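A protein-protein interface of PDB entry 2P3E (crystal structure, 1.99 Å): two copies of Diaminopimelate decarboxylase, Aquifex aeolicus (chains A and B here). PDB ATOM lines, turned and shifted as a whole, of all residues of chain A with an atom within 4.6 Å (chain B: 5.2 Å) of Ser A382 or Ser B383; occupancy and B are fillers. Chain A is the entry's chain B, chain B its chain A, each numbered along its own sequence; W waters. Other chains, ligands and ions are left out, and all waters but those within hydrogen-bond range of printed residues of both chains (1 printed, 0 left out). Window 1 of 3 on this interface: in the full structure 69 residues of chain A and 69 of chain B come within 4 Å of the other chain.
NH1 of Arg A390 is in hydrogen-bond range of ND1 of His B384, at 3.0 Å.
O of Asn B314 is in hydrogen-bond range of OG of Ser B382 (2.6 Å). N of Ser B383 is in hydrogen-bond range of O of Asn B314. The backbone carbonyl oxygen (O) of Ser B382 lies within hydrogen-bond range of the guanidinium group (NH2) of Arg B390 (3.1 Å). The side-chain hydroxyl of Ser B383 is in hydrogen-bond range of the backbone NH of Tyr B385, 3.2 Å away. The backbone carbonyl oxygen (O) of Asn A314 is in hydrogen-bond range of the backbone NH (N) of Ser A383 (3.0 Å). The backbone carbonyl oxygen (O) of Ser A382 lies within hydrogen-bond range of the guanidinium group (NH1) of Arg A390 (3.1 Å).
Ala A380 touches Tyr B385. Met A381 touches Ser B383 (O to CB, 3.96 Å). CG of Met A381 touches CD1 of Tyr B385, 3.7 Å away. Ser B383 touches Ser A382 (CB to O, 3.7 Å). CB of Ser A383 touches O of Ser B382, 3.7 Å away.
Ser A382 touches one residue of chain B. Ser B383 touches just these residues of chain A: Met A381 and Ser A382. Of the printed residues of chain B, Ser A383 touches Ser B382. Printed residues of chain B within 4 Å of Met A381: Ser B383 and Tyr B385. Of the printed residues of chain B, Ala A380 touches Tyr B385. Printed residues of chain B within 4 Å of Arg A390: His B384 (3.0 Å). Asn B314 touches none of the printed residues of chain A. The nearest printed residue of chain B that does not touch Ala A380 is His B384 (4.03 Å).
Of the 9 printed residues of chain A, 5 touch a printed residue of chain B. Among the printed residues, 6 pairs touch across the chains. Among the printed residues, no Asp or Glu carboxylate lies within 4 Å of a Lys or Arg side-chain nitrogen of the other chain.
Met A381 touches Ser B383, but with the chains exchanged Ser A383 does not touch Met B381 (4.2 Å). Ser A382 touches Ser B383, and with the chains exchanged Ser A383 touches Ser B382. 5 positions are printed for both chains.
Water W1 lies within hydrogen-bond range of the backbone carbonyl oxygen (O) of Ser A382 (2.7 Å), the backbone NH (N) of His B384 (2.9 Å), the backbone carbonyl oxygen (O) of Ala A380 (2.9 Å) and the guanidinium group (NH1) of Arg A390 (3.4 Å).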
ATOM      1  N   ASN A 314      -7.973   7.372  34.249  1.00  0.00           N
ATOM      2  CA  ASN A 314      -7.164   8.237  33.392  1.00  0.00           C
ATOM      3  C   ASN A 314      -6.671   7.522  32.145  1.00  0.00           C
ATOM      4  O   ASN A 314      -6.388   8.174  31.135  1.00  0.00           O
ATOM      5  CB  ASN A 314      -5.944   8.765  34.167  1.00  0.00           C
ATOM      6  CG  ASN A 314      -5.035   7.640  34.681  1.00  0.00           C
ATOM      7  OD1 ASN A 314      -5.457   6.749  35.435  1.00  0.00           O
ATOM      8  ND2 ASN A 314      -3.776   7.690  34.287  1.00  0.00           N
ATOM      9  N   ASP A 315      -6.548   6.195  32.236  1.00  0.00           N
ATOM     10  CA  ASP A 315      -6.058   5.346  31.127  1.00  0.00           C
ATOM     11  C   ASP A 315      -7.206   4.698  30.369  1.00  0.00           C
ATOM     12  O   ASP A 315      -7.194   4.649  29.135  1.00  0.00           O
ATOM     13  CB  ASP A 315      -5.118   4.254  31.658  1.00  0.00           C
ATOM     14  CG  ASP A 315      -3.868   4.828  32.323  1.00  0.00           C
ATOM     15  OD1 ASP A 315      -3.036   5.458  31.621  1.00  0.00           O
ATOM     16  OD2 ASP A 315      -3.716   4.644  33.550  1.00  0.00           O
ATOM     17  N   GLY A 378     -10.547   3.713  24.399  1.00  0.00           N
ATOM     18  CA  GLY A 378      -9.643   3.440  25.526  1.00  0.00           C
ATOM     19  C   GLY A 378      -8.658   4.593  25.636  1.00  0.00           C
ATOM     20  O   GLY A 378      -8.923   5.605  26.289  1.00  0.00           O
ATOM     21  N   PHE A 379      -7.534   4.483  24.937  1.00  0.00           N
ATOM     22  CA  PHE A 379      -6.618   5.609  24.893  1.00  0.00           C
ATOM     23  C   PHE A 379      -7.307   6.894  24.422  1.00  0.00           C
ATOM     24  O   PHE A 379      -6.954   7.985  24.867  1.00  0.00           O
ATOM     25  CB  PHE A 379      -5.387   5.341  23.998  1.00  0.00           C
ATOM     26  CG  PHE A 379      -4.288   6.349  24.210  1.00  0.00           C
ATOM     27  CD1 PHE A 379      -3.281   6.107  25.144  1.00  0.00           C
ATOM     28  CD2 PHE A 379      -4.289   7.561  23.518  1.00  0.00           C
ATOM     29  CE1 PHE A 379      -2.257   7.053  25.365  1.00  0.00           C
ATOM     30  CE2 PHE A 379      -3.285   8.527  23.750  1.00  0.00           C
ATOM     31  CZ  PHE A 379      -2.273   8.268  24.676  1.00  0.00           C
ATOM     32  N   ALA A 380      -8.281   6.767  23.529  1.00  0.00           N
ATOM     33  CA  ALA A 380      -8.986   7.914  22.954  1.00  0.00           C
ATOM     34  C   ALA A 380      -9.597   8.848  24.027  1.00  0.00           C
ATOM     35  O   ALA A 380      -9.681  10.063  23.820  1.00  0.00           O
ATOM     36  CB  ALA A 380     -10.055   7.452  21.943  1.00  0.00           C
ATOM     37  N   MET A 381      -9.991   8.275  25.168  1.00  0.00           N
ATOM     38  CA  MET A 381     -10.605   9.048  26.261  1.00  0.00           C
ATOM     39  C   MET A 381      -9.657   9.256  27.452  1.00  0.00           C
ATOM     40  O   MET A 381     -10.063   9.770  28.487  1.00  0.00           O
ATOM     41  CB  MET A 381     -11.915   8.389  26.723  1.00  0.00           C
ATOM     42  CG  MET A 381     -12.914   8.163  25.579  1.00  0.00           C
ATOM     43  SD  MET A 381     -14.521   7.514  26.138  1.00  0.00           S
ATOM     44  CE  MET A 381     -15.368   9.013  26.551  1.00  0.00           C
ATOM     45  N   SER A 382      -8.391   8.869  27.279  1.00  0.00           N
ATOM     46  CA  SER A 382      -7.360   9.008  28.305  1.00  0.00           C
ATOM     47  C   SER A 382      -6.975  10.481  28.554  1.00  0.00           C
ATOM     48  O   SER A 382      -6.819  11.290  27.601  1.00  0.00           O
ATOM     49  CB  SER A 382      -6.129   8.174  27.905  1.00  0.00           C
ATOM     50  OG  SER A 382      -5.122   8.219  28.892  1.00  0.00           O
ATOM     51  N   SER A 383      -6.850  10.831  29.836  1.00  0.00           N
ATOM     52  CA  SER A 383      -6.590  12.217  30.243  1.00  0.00           C
ATOM     53  C   SER A 383      -5.303  12.292  31.071  1.00  0.00           C
ATOM     54  O   SER A 383      -4.553  11.295  31.193  1.00  0.00           O
ATOM     55  CB  SER A 383      -7.778  12.767  31.053  1.00  0.00           C
ATOM     56  OG  SER A 383      -7.802  12.158  32.345  1.00  0.00           O
ATOM     57  N   ARG A 390       0.217   9.749  30.155  1.00  0.00           N
ATOM     58  CA  ARG A 390      -0.488   8.646  29.518  1.00  0.00           C
ATOM     59  C   ARG A 390       0.460   7.529  29.074  1.00  0.00           C
ATOM     60  O   ARG A 390       1.683   7.712  28.988  1.00  0.00           O
ATOM     61  CB  ARG A 390      -1.355   9.135  28.352  1.00  0.00           C
ATOM     62  CG  ARG A 390      -2.475  10.093  28.805  1.00  0.00           C
ATOM     63  CD  ARG A 390      -3.346  10.569  27.653  1.00  0.00           C
ATOM     64  NE  ARG A 390      -2.614  11.460  26.737  1.00  0.00           N
ATOM     65  CZ  ARG A 390      -3.191  12.360  25.945  1.00  0.00           C
ATOM     66  NH1 ARG A 390      -4.516  12.495  25.952  1.00  0.00           N
ATOM     67  NH2 ARG A 390      -2.450  13.124  25.143  1.00  0.00           N
ATOM     68  N   ASN B 314     -15.068  16.908  26.662  1.00  0.00           N
ATOM     69  CA  ASN B 314     -13.605  16.903  26.525  1.00  0.00           C
ATOM     70  C   ASN B 314     -12.959  18.079  27.274  1.00  0.00           C
ATOM     71  O   ASN B 314     -11.800  17.976  27.714  1.00  0.00           O
ATOM     72  CB  ASN B 314     -13.192  16.959  25.048  1.00  0.00           C
ATOM     73  CG  ASN B 314     -13.708  18.206  24.347  1.00  0.00           C
ATOM     74  OD1 ASN B 314     -14.911  18.408  24.216  1.00  0.00           O
ATOM     75  ND2 ASN B 314     -12.801  19.036  23.888  1.00  0.00           N
ATOM     76  N   MET B 381      -9.606  17.336  34.196  1.00  0.00           N
ATOM     77  CA  MET B 381     -10.158  16.079  33.660  1.00  0.00           C
ATOM     78  C   MET B 381     -10.389  16.164  32.142  1.00  0.00           C
ATOM     79  O   MET B 381     -11.069  15.308  31.558  1.00  0.00           O
ATOM     80  CB  MET B 381     -11.473  15.749  34.380  1.00  0.00           C
ATOM     81  CG  MET B 381     -11.332  15.643  35.941  1.00  0.00           C
ATOM     82  SD  MET B 381     -12.906  15.128  36.690  1.00  0.00           S
ATOM     83  CE  MET B 381     -12.891  13.390  36.249  1.00  0.00           C
ATOM     84  N   SER B 382      -9.802  17.188  31.523  1.00  0.00           N
ATOM     85  CA  SER B 382      -9.907  17.440  30.079  1.00  0.00           C
ATOM     86  C   SER B 382      -9.067  16.425  29.289  1.00  0.00           C
ATOM     87  O   SER B 382      -7.908  16.138  29.637  1.00  0.00           O
ATOM     88  CB  SER B 382      -9.456  18.894  29.767  1.00  0.00           C
ATOM     89  OG  SER B 382      -9.691  19.244  28.407  1.00  0.00           O
ATOM     90  N   SER B 383      -9.652  15.900  28.219  1.00  0.00           N
ATOM     91  CA  SER B 383      -9.005  14.892  27.370  1.00  0.00           C
ATOM     92  C   SER B 383      -8.882  15.381  25.917  1.00  0.00           C
ATOM     93  O   SER B 383      -9.208  16.539  25.599  1.00  0.00           O
ATOM     94  CB  SER B 383      -9.787  13.574  27.411  1.00  0.00           C
ATOM     95  OG  SER B 383     -10.928  13.653  26.534  1.00  0.00           O
ATOM     96  N   HIS B 384      -8.411  14.482  25.048  1.00  0.00           N
ATOM     97  CA  HIS B 384      -8.256  14.757  23.612  1.00  0.00           C
ATOM     98  C   HIS B 384      -9.226  13.935  22.781  1.00  0.00           C
ATOM     99  O   HIS B 384      -9.018  13.711  21.599  1.00  0.00           O
ATOM    100  CB  HIS B 384      -6.830  14.465  23.174  1.00  0.00           C
ATOM    101  CG  HIS B 384      -5.833  15.440  23.723  1.00  0.00           C
ATOM    102  ND1 HIS B 384      -4.679  15.045  24.351  1.00  0.00           N
ATOM    103  CD2 HIS B 384      -5.834  16.792  23.747  1.00  0.00           C
ATOM    104  CE1 HIS B 384      -3.998  16.112  24.736  1.00  0.00           C
ATOM    105  NE2 HIS B 384      -4.676  17.186  24.374  1.00  0.00           N
ATOM    106  N   TYR B 385     -10.300  13.485  23.412  1.00  0.00           N
ATOM    107  CA  TYR B 385     -11.306  12.707  22.683  1.00  0.00           C
ATOM    108  C   TYR B 385     -11.785  13.452  21.424  1.00  0.00           C
ATOM    109  O   TYR B 385     -11.972  14.665  21.472  1.00  0.00           O
ATOM    110  CB  TYR B 385     -12.464  12.420  23.615  1.00  0.00           C
ATOM    111  CG  TYR B 385     -13.452  11.395  23.147  1.00  0.00           C
ATOM    112  CD1 TYR B 385     -13.050  10.213  22.493  1.00  0.00           C
ATOM    113  CD2 TYR B 385     -14.802  11.578  23.417  1.00  0.00           C
ATOM    114  CE1 TYR B 385     -13.988   9.267  22.082  1.00  0.00           C
ATOM    115  CE2 TYR B 385     -15.746  10.645  23.015  1.00  0.00           C
ATOM    116  CZ  TYR B 385     -15.339   9.494  22.365  1.00  0.00           C
ATOM    117  OH  TYR B 385     -16.326   8.598  22.007  1.00  0.00           O
ATOM    118  N   ARG B 388      -9.598  16.633  19.718  1.00  0.00           N
ATOM    119  CA  ARG B 388      -9.891  18.017  20.040  1.00  0.00           C
ATOM    120  C   ARG B 388      -8.803  18.584  20.962  1.00  0.00           C
ATOM    121  O   ARG B 388      -8.623  18.109  22.084  1.00  0.00           O
ATOM    122  CB  ARG B 388     -11.258  18.120  20.722  1.00  0.00           C
ATOM    123  CG  ARG B 388     -12.415  17.652  19.835  1.00  0.00           C
ATOM    124  CD  ARG B 388     -13.718  18.421  20.083  1.00  0.00           C
ATOM    125  NE  ARG B 388     -13.710  19.604  19.219  1.00  0.00           N
ATOM    126  CZ  ARG B 388     -14.222  19.668  17.985  1.00  0.00           C
ATOM    127  NH1 ARG B 388     -14.873  18.645  17.444  1.00  0.00           N
ATOM    128  NH2 ARG B 388     -14.094  20.791  17.296  1.00  0.00           N
ATOM    129  N   ARG B 390      -7.060  20.927  23.633  1.00  0.00           N
ATOM    130  CA  ARG B 390      -7.663  21.555  24.797  1.00  0.00           C
ATOM    131  C   ARG B 390      -7.572  23.082  24.744  1.00  0.00           C
ATOM    132  O   ARG B 390      -6.820  23.647  23.933  1.00  0.00           O
ATOM    133  CB  ARG B 390      -7.014  21.076  26.090  1.00  0.00           C
ATOM    134  CG  ARG B 390      -7.114  19.590  26.360  1.00  0.00           C
ATOM    135  CD  ARG B 390      -5.734  19.287  26.931  1.00  0.00           C
ATOM    136  NE  ARG B 390      -5.755  18.299  27.918  1.00  0.00           N
ATOM    137  CZ  ARG B 390      -4.686  17.698  28.404  1.00  0.00           C
ATOM    138  NH1 ARG B 390      -3.440  17.986  27.991  1.00  0.00           N
ATOM    139  NH2 ARG B 390      -4.904  16.777  29.302  1.00  0.00           N
HETATM  140  O   HOH W   1      -7.673  11.714  25.042  1.00  0.00           O
